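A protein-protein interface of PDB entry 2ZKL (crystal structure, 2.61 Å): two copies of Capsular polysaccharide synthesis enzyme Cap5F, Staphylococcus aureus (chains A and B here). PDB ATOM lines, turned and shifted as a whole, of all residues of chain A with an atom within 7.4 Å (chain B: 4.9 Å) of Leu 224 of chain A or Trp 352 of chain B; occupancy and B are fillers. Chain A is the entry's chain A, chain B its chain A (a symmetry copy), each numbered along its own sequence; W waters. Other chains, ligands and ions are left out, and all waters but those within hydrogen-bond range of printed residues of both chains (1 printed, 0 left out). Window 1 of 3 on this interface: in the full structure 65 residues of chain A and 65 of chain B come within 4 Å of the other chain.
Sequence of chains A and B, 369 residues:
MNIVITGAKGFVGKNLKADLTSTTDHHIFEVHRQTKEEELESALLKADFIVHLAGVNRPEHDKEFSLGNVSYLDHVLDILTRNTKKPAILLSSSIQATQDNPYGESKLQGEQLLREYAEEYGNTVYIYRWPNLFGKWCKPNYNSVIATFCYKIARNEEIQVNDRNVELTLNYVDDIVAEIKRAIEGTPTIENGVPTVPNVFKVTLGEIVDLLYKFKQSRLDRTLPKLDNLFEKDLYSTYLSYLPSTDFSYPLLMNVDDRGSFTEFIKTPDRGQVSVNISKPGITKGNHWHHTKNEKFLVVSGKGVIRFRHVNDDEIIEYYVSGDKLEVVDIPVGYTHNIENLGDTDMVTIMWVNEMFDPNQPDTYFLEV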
ATOM      1  N   LYS A 214      -8.827  19.508 -23.814  1.00  0.00           N
ATOM      2  CA  LYS A 214     -10.226  19.727 -23.502  1.00  0.00           C
ATOM      3  C   LYS A 214     -10.494  19.268 -22.072  1.00  0.00           C
ATOM      4  O   LYS A 214     -11.234  19.911 -21.341  1.00  0.00           O
ATOM      5  CB  LYS A 214     -11.136  18.947 -24.444  1.00  0.00           C
ATOM      6  CG  LYS A 214     -12.604  19.162 -24.108  1.00  0.00           C
ATOM      7  CD  LYS A 214     -13.560  18.419 -25.014  1.00  0.00           C
ATOM      8  CE  LYS A 214     -13.786  16.991 -24.552  1.00  0.00           C
ATOM      9  NZ  LYS A 214     -15.019  16.442 -25.171  1.00  0.00           N
ATOM     10  N   PHE A 215      -9.886  18.155 -21.671  1.00  0.00           N
ATOM     11  CA  PHE A 215     -10.089  17.639 -20.328  1.00  0.00           C
ATOM     12  C   PHE A 215      -9.627  18.646 -19.284  1.00  0.00           C
ATOM     13  O   PHE A 215     -10.294  18.844 -18.269  1.00  0.00           O
ATOM     14  CB  PHE A 215      -9.330  16.319 -20.110  1.00  0.00           C
ATOM     15  CG  PHE A 215      -9.810  15.170 -20.960  1.00  0.00           C
ATOM     16  CD1 PHE A 215     -11.067  15.183 -21.553  1.00  0.00           C
ATOM     17  CD2 PHE A 215      -9.000  14.044 -21.136  1.00  0.00           C
ATOM     18  CE1 PHE A 215     -11.520  14.094 -22.309  1.00  0.00           C
ATOM     19  CE2 PHE A 215      -9.436  12.950 -21.885  1.00  0.00           C
ATOM     20  CZ  PHE A 215     -10.705  12.975 -22.477  1.00  0.00           C
ATOM     21  N   SER A 218     -11.857  21.723 -19.221  1.00  0.00           N
ATOM     22  CA  SER A 218     -13.207  21.406 -18.778  1.00  0.00           C
ATOM     23  C   SER A 218     -13.367  21.743 -17.313  1.00  0.00           C
ATOM     24  O   SER A 218     -14.479  21.861 -16.807  1.00  0.00           O
ATOM     25  CB  SER A 218     -13.515  19.927 -19.000  1.00  0.00           C
ATOM     26  OG  SER A 218     -13.776  19.679 -20.369  1.00  0.00           O
ATOM     27  N   ARG A 219     -12.241  21.897 -16.635  1.00  0.00           N
ATOM     28  CA  ARG A 219     -12.241  22.223 -15.222  1.00  0.00           C
ATOM     29  C   ARG A 219     -12.865  23.606 -15.053  1.00  0.00           C
ATOM     30  O   ARG A 219     -13.696  23.818 -14.175  1.00  0.00           O
ATOM     31  CB  ARG A 219     -10.805  22.232 -14.702  1.00  0.00           C
ATOM     32  CG  ARG A 219     -10.680  22.167 -13.196  1.00  0.00           C
ATOM     33  CD  ARG A 219     -10.176  20.800 -12.750  1.00  0.00           C
ATOM     34  NE  ARG A 219      -8.994  20.938 -11.917  1.00  0.00           N
ATOM     35  CZ  ARG A 219      -8.469  19.963 -11.187  1.00  0.00           C
ATOM     36  NH1 ARG A 219      -9.013  18.754 -11.181  1.00  0.00           N
ATOM     37  NH2 ARG A 219      -7.406  20.208 -10.434  1.00  0.00           N
ATOM     38  N   ASP A 221     -14.710  25.576 -17.557  1.00  0.00           N
ATOM     39  CA  ASP A 221     -16.072  25.747 -18.034  1.00  0.00           C
ATOM     40  C   ASP A 221     -17.065  24.690 -17.562  1.00  0.00           C
ATOM     41  O   ASP A 221     -18.111  24.510 -18.179  1.00  0.00           O
ATOM     42  CB  ASP A 221     -16.102  25.856 -19.560  1.00  0.00           C
ATOM     43  CG  ASP A 221     -15.187  24.873 -20.232  1.00  0.00           C
ATOM     44  OD1 ASP A 221     -15.350  23.659 -19.994  1.00  0.00           O
ATOM     45  OD2 ASP A 221     -14.305  25.312 -21.004  1.00  0.00           O
ATOM     46  N   ARG A 222     -16.739  24.017 -16.457  1.00  0.00           N
ATOM     47  CA  ARG A 222     -17.592  22.982 -15.861  1.00  0.00           C
ATOM     48  C   ARG A 222     -18.104  21.961 -16.888  1.00  0.00           C
ATOM     49  O   ARG A 222     -19.209  21.450 -16.776  1.00  0.00           O
ATOM     50  CB  ARG A 222     -18.791  23.627 -15.149  1.00  0.00           C
ATOM     51  CG  ARG A 222     -18.496  24.951 -14.443  1.00  0.00           C
ATOM     52  CD  ARG A 222     -17.350  24.855 -13.452  1.00  0.00           C
ATOM     53  NE  ARG A 222     -17.040  26.163 -12.881  1.00  0.00           N
ATOM     54  CZ  ARG A 222     -15.911  26.459 -12.240  1.00  0.00           C
ATOM     55  NH1 ARG A 222     -14.970  25.541 -12.088  1.00  0.00           N
ATOM     56  NH2 ARG A 222     -15.722  27.673 -11.740  1.00  0.00           N
ATOM     57  N   THR A 223     -17.277  21.665 -17.878  1.00  0.00           N
ATOM     58  CA  THR A 223     -17.614  20.734 -18.947  1.00  0.00           C
ATOM     59  C   THR A 223     -17.368  19.253 -18.607  1.00  0.00           C
ATOM     60  O   THR A 223     -16.645  18.927 -17.656  1.00  0.00           O
ATOM     61  CB  THR A 223     -16.837  21.163 -20.221  1.00  0.00           C
ATOM     62  OG1 THR A 223     -17.655  22.081 -20.946  1.00  0.00           O
ATOM     63  CG2 THR A 223     -16.470  19.984 -21.115  1.00  0.00           C
ATOM     64  N   LEU A 224     -17.982  18.364 -19.385  1.00  0.00           N
ATOM     65  CA  LEU A 224     -17.844  16.919 -19.183  1.00  0.00           C
ATOM     66  C   LEU A 224     -17.395  16.165 -20.444  1.00  0.00           C
ATOM     67  O   LEU A 224     -17.637  16.607 -21.568  1.00  0.00           O
ATOM     68  CB  LEU A 224     -19.174  16.353 -18.676  1.00  0.00           C
ATOM     69  CG  LEU A 224     -19.373  16.180 -17.160  1.00  0.00           C
ATOM     70  CD1 LEU A 224     -18.520  17.141 -16.385  1.00  0.00           C
ATOM     71  CD2 LEU A 224     -20.850  16.348 -16.819  1.00  0.00           C
ATOM     72  N   PRO A 225     -16.724  15.017 -20.271  1.00  0.00           N
ATOM     73  CA  PRO A 225     -16.248  14.214 -21.410  1.00  0.00           C
ATOM     74  C   PRO A 225     -17.419  13.492 -22.079  1.00  0.00           C
ATOM     75  O   PRO A 225     -18.438  13.261 -21.433  1.00  0.00           O
ATOM     76  CB  PRO A 225     -15.290  13.211 -20.757  1.00  0.00           C
ATOM     77  CG  PRO A 225     -14.996  13.783 -19.402  1.00  0.00           C
ATOM     78  CD  PRO A 225     -16.285  14.421 -19.000  1.00  0.00           C
ATOM     79  N   LYS A 226     -17.309  13.156 -23.363  1.00  0.00           N
ATOM     80  CA  LYS A 226     -18.407  12.418 -23.980  1.00  0.00           C
ATOM     81  C   LYS A 226     -18.196  10.965 -23.564  1.00  0.00           C
ATOM     82  O   LYS A 226     -17.447  10.221 -24.190  1.00  0.00           O
ATOM     83  CB  LYS A 226     -18.422  12.533 -25.507  1.00  0.00           C
ATOM     84  CG  LYS A 226     -19.860  12.457 -26.043  1.00  0.00           C
ATOM     85  CD  LYS A 226     -19.952  12.190 -27.539  1.00  0.00           C
ATOM     86  CE  LYS A 226     -21.335  12.567 -28.097  1.00  0.00           C
ATOM     87  NZ  LYS A 226     -22.504  11.927 -27.403  1.00  0.00           N
ATOM     88  N   LEU A 227     -18.876  10.579 -22.495  1.00  0.00           N
ATOM     89  CA  LEU A 227     -18.744   9.256 -21.921  1.00  0.00           C
ATOM     90  C   LEU A 227     -19.248   8.035 -22.690  1.00  0.00           C
ATOM     91  O   LEU A 227     -19.015   6.903 -22.256  1.00  0.00           O
ATOM     92  CB  LEU A 227     -19.339   9.269 -20.518  1.00  0.00           C
ATOM     93  CG  LEU A 227     -18.397   9.691 -19.385  1.00  0.00           C
ATOM     94  CD1 LEU A 227     -17.020  10.075 -19.931  1.00  0.00           C
ATOM     95  CD2 LEU A 227     -19.032  10.823 -18.601  1.00  0.00           C
ATOM     96  N   GLU A 232     -12.488   8.078 -25.412  1.00  0.00           N
ATOM     97  CA  GLU A 232     -12.510   9.325 -24.653  1.00  0.00           C
ATOM     98  C   GLU A 232     -12.697   9.016 -23.179  1.00  0.00           C
ATOM     99  O   GLU A 232     -12.009   9.578 -22.316  1.00  0.00           O
ATOM    100  CB  GLU A 232     -13.643  10.231 -25.142  1.00  0.00           C
ATOM    101  CG  GLU A 232     -13.684  11.588 -24.444  1.00  0.00           C
ATOM    102  CD  GLU A 232     -14.496  12.627 -25.203  1.00  0.00           C
ATOM    103  OE1 GLU A 232     -14.700  12.454 -26.422  1.00  0.00           O
ATOM    104  OE2 GLU A 232     -14.914  13.629 -24.585  1.00  0.00           O
ATOM    105  N   TYR A 236      -9.980   9.914 -20.451  1.00  0.00           N
ATOM    106  CA  TYR A 236     -10.290  10.840 -19.375  1.00  0.00           C
ATOM    107  C   TYR A 236      -9.828  10.278 -18.038  1.00  0.00           C
ATOM    108  O   TYR A 236      -9.168  10.974 -17.259  1.00  0.00           O
ATOM    109  CB  TYR A 236     -11.793  11.141 -19.326  1.00  0.00           C
ATOM    110  CG  TYR A 236     -12.173  12.089 -18.215  1.00  0.00           C
ATOM    111  CD1 TYR A 236     -11.659  13.382 -18.168  1.00  0.00           C
ATOM    112  CD2 TYR A 236     -13.031  11.684 -17.189  1.00  0.00           C
ATOM    113  CE1 TYR A 236     -11.988  14.260 -17.112  1.00  0.00           C
ATOM    114  CE2 TYR A 236     -13.369  12.547 -16.139  1.00  0.00           C
ATOM    115  CZ  TYR A 236     -12.841  13.833 -16.103  1.00  0.00           C
ATOM    116  OH  TYR A 236     -13.132  14.671 -15.037  1.00  0.00           O
ATOM    117  N   LEU A 240      -6.869  11.848 -15.457  1.00  0.00           N
ATOM    118  CA  LEU A 240      -7.067  12.154 -14.045  1.00  0.00           C
ATOM    119  C   LEU A 240      -5.975  11.539 -13.174  1.00  0.00           C
ATOM    120  O   LEU A 240      -5.582  12.126 -12.164  1.00  0.00           O
ATOM    121  CB  LEU A 240      -8.430  11.633 -13.579  1.00  0.00           C
ATOM    122  CG  LEU A 240      -9.600  12.600 -13.377  1.00  0.00           C
ATOM    123  CD1 LEU A 240      -9.498  13.780 -14.320  1.00  0.00           C
ATOM    124  CD2 LEU A 240     -10.908  11.847 -13.586  1.00  0.00           C
ATOM    125  N   TYR A 250     -10.889  21.999  -7.293  1.00  0.00           N
ATOM    126  CA  TYR A 250     -10.944  23.300  -7.922  1.00  0.00           C
ATOM    127  C   TYR A 250     -12.146  24.072  -7.380  1.00  0.00           C
ATOM    128  O   TYR A 250     -13.195  23.493  -7.079  1.00  0.00           O
ATOM    129  CB  TYR A 250     -11.017  23.182  -9.451  1.00  0.00           C
ATOM    130  CG  TYR A 250     -12.141  22.330  -9.982  1.00  0.00           C
ATOM    131  CD1 TYR A 250     -12.055  20.939  -9.964  1.00  0.00           C
ATOM    132  CD2 TYR A 250     -13.286  22.913 -10.524  1.00  0.00           C
ATOM    133  CE1 TYR A 250     -13.079  20.148 -10.479  1.00  0.00           C
ATOM    134  CE2 TYR A 250     -14.319  22.127 -11.042  1.00  0.00           C
ATOM    135  CZ  TYR A 250     -14.207  20.744 -11.017  1.00  0.00           C
ATOM    136  OH  TYR A 250     -15.207  19.958 -11.539  1.00  0.00           O
ATOM    137  N   PHE A 265     -22.379  23.898 -11.290  1.00  0.00           N
ATOM    138  CA  PHE A 265     -21.573  22.728 -10.974  1.00  0.00           C
ATOM    139  C   PHE A 265     -21.080  21.958 -12.202  1.00  0.00           C
ATOM    140  O   PHE A 265     -19.873  21.771 -12.386  1.00  0.00           O
ATOM    141  CB  PHE A 265     -22.390  21.806 -10.064  1.00  0.00           C
ATOM    142  CG  PHE A 265     -21.749  20.476  -9.795  1.00  0.00           C
ATOM    143  CD1 PHE A 265     -20.371  20.362  -9.642  1.00  0.00           C
ATOM    144  CD2 PHE A 265     -22.536  19.333  -9.669  1.00  0.00           C
ATOM    145  CE1 PHE A 265     -19.782  19.119  -9.366  1.00  0.00           C
ATOM    146  CE2 PHE A 265     -21.960  18.084  -9.392  1.00  0.00           C
ATOM    147  CZ  PHE A 265     -20.581  17.980  -9.240  1.00  0.00           C
ATOM    148  N   ILE A 266     -22.032  21.531 -13.032  1.00  0.00           N
ATOM    149  CA  ILE A 266     -21.771  20.752 -14.221  1.00  0.00           C
ATOM    150  C   ILE A 266     -22.592  21.267 -15.418  1.00  0.00           C
ATOM    151  O   ILE A 266     -23.798  21.474 -15.307  1.00  0.00           O
ATOM    152  CB  ILE A 266     -22.083  19.267 -13.893  1.00  0.00           C
ATOM    153  CG1 ILE A 266     -20.781  18.491 -13.801  1.00  0.00           C
ATOM    154  CG2 ILE A 266     -23.017  18.646 -14.902  1.00  0.00           C
ATOM    155  CD1 ILE A 266     -19.926  18.900 -12.658  1.00  0.00           C
ATOM    156  N   LYS A 267     -21.929  21.472 -16.557  1.00  0.00           N
ATOM    157  CA  LYS A 267     -22.581  21.964 -17.773  1.00  0.00           C
ATOM    158  C   LYS A 267     -22.368  21.037 -18.978  1.00  0.00           C
ATOM    159  O   LYS A 267     -21.270  20.547 -19.203  1.00  0.00           O
ATOM    160  CB  LYS A 267     -22.049  23.364 -18.129  1.00  0.00           C
ATOM    161  CG  LYS A 267     -22.263  24.415 -17.044  1.00  0.00           C
ATOM    162  CD  LYS A 267     -22.746  25.744 -17.618  1.00  0.00           C
ATOM    163  CE  LYS A 267     -21.610  26.627 -18.093  1.00  0.00           C
ATOM    164  NZ  LYS A 267     -20.977  27.311 -16.939  1.00  0.00           N
ATOM    165  N   THR A 268     -23.419  20.796 -19.753  1.00  0.00           N
ATOM    166  CA  THR A 268     -23.303  19.950 -20.937  1.00  0.00           C
ATOM    167  C   THR A 268     -24.173  20.496 -22.066  1.00  0.00           C
ATOM    168  O   THR A 268     -25.204  21.119 -21.831  1.00  0.00           O
ATOM    169  CB  THR A 268     -23.759  18.478 -20.685  1.00  0.00           C
ATOM    170  OG1 THR A 268     -25.192  18.411 -20.670  1.00  0.00           O
ATOM    171  CG2 THR A 268     -23.218  17.962 -19.371  1.00  0.00           C
ATOM    172  N   PRO A 269     -23.767  20.261 -23.314  1.00  0.00           N
ATOM    173  CA  PRO A 269     -24.570  20.759 -24.432  1.00  0.00           C
ATOM    174  C   PRO A 269     -25.732  19.832 -24.791  1.00  0.00           C
ATOM    175  O   PRO A 269     -26.616  20.213 -25.563  1.00  0.00           O
ATOM    176  CB  PRO A 269     -23.544  20.862 -25.566  1.00  0.00           C
ATOM    177  CG  PRO A 269     -22.635  19.694 -25.273  1.00  0.00           C
ATOM    178  CD  PRO A 269     -22.441  19.803 -23.773  1.00  0.00           C
ATOM    179  N   GLY A 272     -28.327  19.087 -20.402  1.00  0.00           N
ATOM    180  CA  GLY A 272     -28.563  20.134 -19.435  1.00  0.00           C
ATOM    181  C   GLY A 272     -27.372  20.397 -18.552  1.00  0.00           C
ATOM    182  O   GLY A 272     -26.242  20.021 -18.869  1.00  0.00           O
ATOM    183  N   VAL A 274     -26.399  21.271 -14.081  1.00  0.00           N
ATOM    184  CA  VAL A 274     -26.931  21.313 -12.728  1.00  0.00           C
ATOM    185  C   VAL A 274     -26.172  22.335 -11.876  1.00  0.00           C
ATOM    186  O   VAL A 274     -24.941  22.424 -11.925  1.00  0.00           O
ATOM    187  CB  VAL A 274     -26.941  19.895 -12.037  1.00  0.00           C
ATOM    188  CG1 VAL A 274     -26.587  18.811 -13.035  1.00  0.00           C
ATOM    189  CG2 VAL A 274     -26.029  19.876 -10.833  1.00  0.00           C
ATOM    190  N   ARG B 271     -23.051  11.309 -20.160  1.00  0.00           N
ATOM    191  CA  ARG B 271     -22.429  12.383 -19.397  1.00  0.00           C
ATOM    192  C   ARG B 271     -22.454  12.077 -17.919  1.00  0.00           C
ATOM    193  O   ARG B 271     -22.426  12.982 -17.079  1.00  0.00           O
ATOM    194  CB  ARG B 271     -23.132  13.721 -19.676  1.00  0.00           C
ATOM    195  CG  ARG B 271     -23.558  13.836 -21.099  1.00  0.00           C
ATOM    196  CD  ARG B 271     -23.025  15.049 -21.838  1.00  0.00           C
ATOM    197  NE  ARG B 271     -21.605  15.076 -22.126  1.00  0.00           N
ATOM    198  CZ  ARG B 271     -21.092  15.554 -23.265  1.00  0.00           C
ATOM    199  NH1 ARG B 271     -21.893  16.016 -24.217  1.00  0.00           N
ATOM    200  NH2 ARG B 271     -19.775  15.632 -23.440  1.00  0.00           N
ATOM    201  N   GLY B 272     -22.503  10.790 -17.604  1.00  0.00           N
ATOM    202  CA  GLY B 272     -22.491  10.379 -16.218  1.00  0.00           C
ATOM    203  C   GLY B 272     -23.830  10.537 -15.548  1.00  0.00           C
ATOM    204  O   GLY B 272     -24.868  10.650 -16.203  1.00  0.00           O
ATOM    205  N   GLN B 273     -23.804  10.530 -14.225  1.00  0.00           N
ATOM    206  CA  GLN B 273     -25.012  10.668 -13.453  1.00  0.00           C
ATOM    207  C   GLN B 273     -24.630  11.380 -12.171  1.00  0.00           C
ATOM    208  O   GLN B 273     -23.444  11.435 -11.833  1.00  0.00           O
ATOM    209  CB  GLN B 273     -25.601   9.291 -13.149  1.00  0.00           C
ATOM    210  CG  GLN B 273     -24.719   8.398 -12.321  1.00  0.00           C
ATOM    211  CD  GLN B 273     -25.368   7.044 -12.032  1.00  0.00           C
ATOM    212  OE1 GLN B 273     -25.551   6.226 -12.941  1.00  0.00           O
ATOM    213  NE2 GLN B 273     -25.726   6.807 -10.763  1.00  0.00           N
ATOM    214  N   VAL B 274     -25.614  11.970 -11.490  1.00  0.00           N
ATOM    215  CA  VAL B 274     -25.330  12.636 -10.228  1.00  0.00           C
ATOM    216  C   VAL B 274     -26.275  12.142  -9.129  1.00  0.00           C
ATOM    217  O   VAL B 274     -27.481  11.982  -9.342  1.00  0.00           O
ATOM    218  CB  VAL B 274     -25.375  14.208 -10.349  1.00  0.00           C
ATOM    219  CG1 VAL B 274     -25.496  14.629 -11.800  1.00  0.00           C
ATOM    220  CG2 VAL B 274     -26.482  14.783  -9.498  1.00  0.00           C
ATOM    221  N   ASN B 294     -14.674   7.167 -11.952  1.00  0.00           N
ATOM    222  CA  ASN B 294     -14.144   8.336 -11.274  1.00  0.00           C
ATOM    223  C   ASN B 294     -15.280   9.281 -10.941  1.00  0.00           C
ATOM    224  O   ASN B 294     -16.331   9.279 -11.598  1.00  0.00           O
ATOM    225  CB  ASN B 294     -13.048   9.043 -12.092  1.00  0.00           C
ATOM    226  CG  ASN B 294     -13.568   9.721 -13.340  1.00  0.00           C
ATOM    227  OD1 ASN B 294     -13.574   9.136 -14.421  1.00  0.00           O
ATOM    228  ND2 ASN B 294     -13.999  10.964 -13.200  1.00  0.00           N
ATOM    229  N   GLU B 295     -15.075  10.092  -9.913  1.00  0.00           N
ATOM    230  CA  GLU B 295     -16.125  10.987  -9.479  1.00  0.00           C
ATOM    231  C   GLU B 295     -15.741  12.432  -9.234  1.00  0.00           C
ATOM    232  O   GLU B 295     -14.581  12.831  -9.368  1.00  0.00           O
ATOM    233  CB  GLU B 295     -16.732  10.411  -8.215  1.00  0.00           C
ATOM    234  CG  GLU B 295     -17.045   8.941  -8.360  1.00  0.00           C
ATOM    235  CD  GLU B 295     -16.715   8.157  -7.115  1.00  0.00           C
ATOM    236  OE1 GLU B 295     -15.510   7.910  -6.863  1.00  0.00           O
ATOM    237  OE2 GLU B 295     -17.669   7.799  -6.383  1.00  0.00           O
ATOM    238  N   LYS B 296     -16.758  13.211  -8.886  1.00  0.00           N
ATOM    239  CA  LYS B 296     -16.608  14.615  -8.557  1.00  0.00           C
ATOM    240  C   LYS B 296     -17.466  14.810  -7.312  1.00  0.00           C
ATOM    241  O   LYS B 296     -18.678  14.663  -7.374  1.00  0.00           O
ATOM    242  CB  LYS B 296     -17.122  15.502  -9.695  1.00  0.00           C
ATOM    243  CG  LYS B 296     -16.124  15.774 -10.806  1.00  0.00           C
ATOM    244  CD  LYS B 296     -16.812  16.561 -11.919  1.00  0.00           C
ATOM    245  CE  LYS B 296     -15.943  16.749 -13.151  1.00  0.00           C
ATOM    246  NZ  LYS B 296     -14.669  17.420 -12.840  1.00  0.00           N
ATOM    247  N   ILE B 350     -22.862  16.181  -3.099  1.00  0.00           N
ATOM    248  CA  ILE B 350     -23.393  15.880  -4.414  1.00  0.00           C
ATOM    249  C   ILE B 350     -22.262  15.115  -5.069  1.00  0.00           C
ATOM    250  O   ILE B 350     -21.096  15.527  -4.996  1.00  0.00           O
ATOM    251  CB  ILE B 350     -23.697  17.153  -5.213  1.00  0.00           C
ATOM    252  CG1 ILE B 350     -24.671  18.030  -4.428  1.00  0.00           C
ATOM    253  CG2 ILE B 350     -24.295  16.787  -6.565  1.00  0.00           C
ATOM    254  CD1 ILE B 350     -25.952  17.320  -4.030  1.00  0.00           C
ATOM    255  N   MET B 351     -22.602  13.992  -5.687  1.00  0.00           N
ATOM    256  CA  MET B 351     -21.599  13.158  -6.321  1.00  0.00           C
ATOM    257  C   MET B 351     -21.891  12.914  -7.797  1.00  0.00           C
ATOM    258  O   MET B 351     -22.952  12.399  -8.162  1.00  0.00           O
ATOM    259  CB  MET B 351     -21.495  11.809  -5.569  1.00  0.00           C
ATOM    260  CG  MET B 351     -20.897  11.908  -4.145  1.00  0.00           C
ATOM    261  SD  MET B 351     -20.812  10.372  -3.140  1.00  0.00           S
ATOM    262  CE  MET B 351     -20.180   9.203  -4.331  1.00  0.00           C
ATOM    263  N   TRP B 352     -20.963  13.320  -8.653  1.00  0.00           N
ATOM    264  CA  TRP B 352     -21.109  13.062 -10.072  1.00  0.00           C
ATOM    265  C   TRP B 352     -20.191  11.874 -10.362  1.00  0.00           C
ATOM    266  O   TRP B 352     -19.061  11.833  -9.873  1.00  0.00           O
ATOM    267  CB  TRP B 352     -20.649  14.241 -10.924  1.00  0.00           C
ATOM    268  CG  TRP B 352     -20.678  13.899 -12.401  1.00  0.00           C
ATOM    269  CD1 TRP B 352     -21.762  13.940 -13.235  1.00  0.00           C
ATOM    270  CD2 TRP B 352     -19.583  13.411 -13.195  1.00  0.00           C
ATOM    271  NE1 TRP B 352     -21.410  13.511 -14.496  1.00  0.00           N
ATOM    272  CE2 TRP B 352     -20.080  13.182 -14.498  1.00  0.00           C
ATOM    273  CE3 TRP B 352     -18.235  13.146 -12.930  1.00  0.00           C
ATOM    274  CZ2 TRP B 352     -19.269  12.705 -15.538  1.00  0.00           C
ATOM    275  CZ3 TRP B 352     -17.427  12.668 -13.975  1.00  0.00           C
ATOM    276  CH2 TRP B 352     -17.951  12.455 -15.255  1.00  0.00           C
ATOM    277  N   VAL B 353     -20.674  10.918 -11.145  1.00  0.00           N
ATOM    278  CA  VAL B 353     -19.863   9.761 -11.492  1.00  0.00           C
ATOM    279  C   VAL B 353     -19.887   9.581 -13.012  1.00  0.00           C
ATOM    280  O   VAL B 353     -20.894   9.848 -13.661  1.00  0.00           O
ATOM    281  CB  VAL B 353     -20.362   8.491 -10.760  1.00  0.00           C
ATOM    282  CG1 VAL B 353     -21.724   8.125 -11.241  1.00  0.00           C
ATOM    283  CG2 VAL B 353     -19.380   7.354 -10.955  1.00  0.00           C
ATOM    284  N   ASN B 354     -18.768   9.135 -13.574  1.00  0.00           N
ATOM    285  CA  ASN B 354     -18.635   8.976 -15.014  1.00  0.00           C
ATOM    286  C   ASN B 354     -19.350   7.781 -15.640  1.00  0.00           C
ATOM    287  O   ASN B 354     -19.304   7.611 -16.855  1.00  0.00           O
ATOM    288  CB  ASN B 354     -17.152   8.923 -15.376  1.00  0.00           C
ATOM    289  CG  ASN B 354     -16.498   7.611 -14.968  1.00  0.00           C
ATOM    290  OD1 ASN B 354     -16.807   7.041 -13.921  1.00  0.00           O
ATOM    291  ND2 ASN B 354     -15.582   7.134 -15.794  1.00  0.00           N
HETATM  292  O   HOH W   1     -17.896  17.006 -25.473  1.00  0.00           O
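Water W1 lies within hydrogen-bond range of NZ of Lys 214 of chain A and NH2 of Arg 271 of chain B.
The guanidinium group (NH2) of Arg 271 of chain B lies within hydrogen-bond range of the backbone carbonyl oxygen (O) of Leu 224 of chain A (3.0 Å). The backbone carbonyl oxygen of Pro 225 of chain A is in hydrogen-bond range of the guanidinium group of Arg 271 of chain B. OH of Tyr 250 of chain A lies within hydrogen-bond range of NZ of Lys 296 of chain B (2.9 Å). NH2 of Arg 271 of chain B sits close to N of Lys 226 of chain A (3.5 Å).
Of the 12 printed residues of chain B, 7 touch a printed residue of chain A. Along chain B the printed residues that touch a printed residue of chain A span positions 271 to 354. Among the printed residues, no Asp or Glu carboxylate lies within 4 Å of a Lys or Arg side-chain nitrogen of the other chain.
N of Phe 265 of chain A sits at hydrogen-bond distance from O of Val 274 of chain A (3.0 Å). The backbone carbonyl oxygen of Ile 266 of chain A sits at hydrogen-bond distance from the backbone NH of Val 274 of chain A (2.9 Å). OG1 of Thr 268 of chain A sits at hydrogen-bond distance from O of Gly 272 of chain A, at 2.6 Å. The backbone carbonyl oxygen (O) of Arg 271 of chain B sits at hydrogen-bond distance from the indole nitrogen (NE1) of Trp 352 of chain B (2.8 Å). N of Asn 294 of chain B sits at hydrogen-bond distance from OD1 of Asn 354 of chain B (2.9 Å). The backbone NH (N) of Lys 296 of chain B sits at hydrogen-bond distance from the backbone carbonyl oxygen (O) of Trp 352 of chain B.
Of chain A, only Leu 224 and Leu 227 come within 4 Å of Trp 352 of chain B. Of the printed residues of chain A, Arg 271 of chain B touches Leu 224, Pro 225, Lys 226, Leu 227, Thr 268 and Pro 269. Printed residues of chain B within 4 Å of Ile 266 of chain A: Lys 296. Printed residues of chain B within 4 Å of Leu 227 of chain A: Arg 271, Gly 272, Trp 352 and Asn 354. Printed residues of chain A within 4 Å of Lys 296 of chain B: Tyr 236, Tyr 250 and Ile 266. Of the printed residues of chain A, Gly 272 of chain B touches Leu 227 (3.6 Å). Asp 221 of chain A touches none of the printed residues of chain B. Thr 223 of chain A touches none of the printed residues of chain B. The nearest residue of chain A that does not touch Trp 352 of chain B is Phe 265 of chain A (4.1 Å).
2 positions are printed for both chains.
Among the printed residues, pairs that only touch across the chains: Leu 224 of chain A with Trp 352 of chain B (3.7 Å), Leu 227 of chain A with Arg 271 of chain B (3.7 Å), Leu 227 of chain A with Gly 272 of chain B (3.6 Å), Leu 227 of chain A with Trp 352 of chain B (3.6 Å), Leu 227 of chain A with Asn 354 of chain B (3.4 Å), Tyr 236 of chain A with Asn 294 of chain B (3.4 Å), Tyr 236 of chain A with Lys 296 of chain B (3.8 Å), Leu 240 of chain A with Asn 294 of chain B (3.2 Å), Phe 265 of chain A with Ile 350 of chain B (3.9 Å), Ile 266 of chain A with Lys 296 of chain B (3.96 Å), Thr 268 of chain A with Arg 271 of chain B (3.7 Å) and Pro 269 of chain A with Arg 271 of chain B (3.9 Å).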
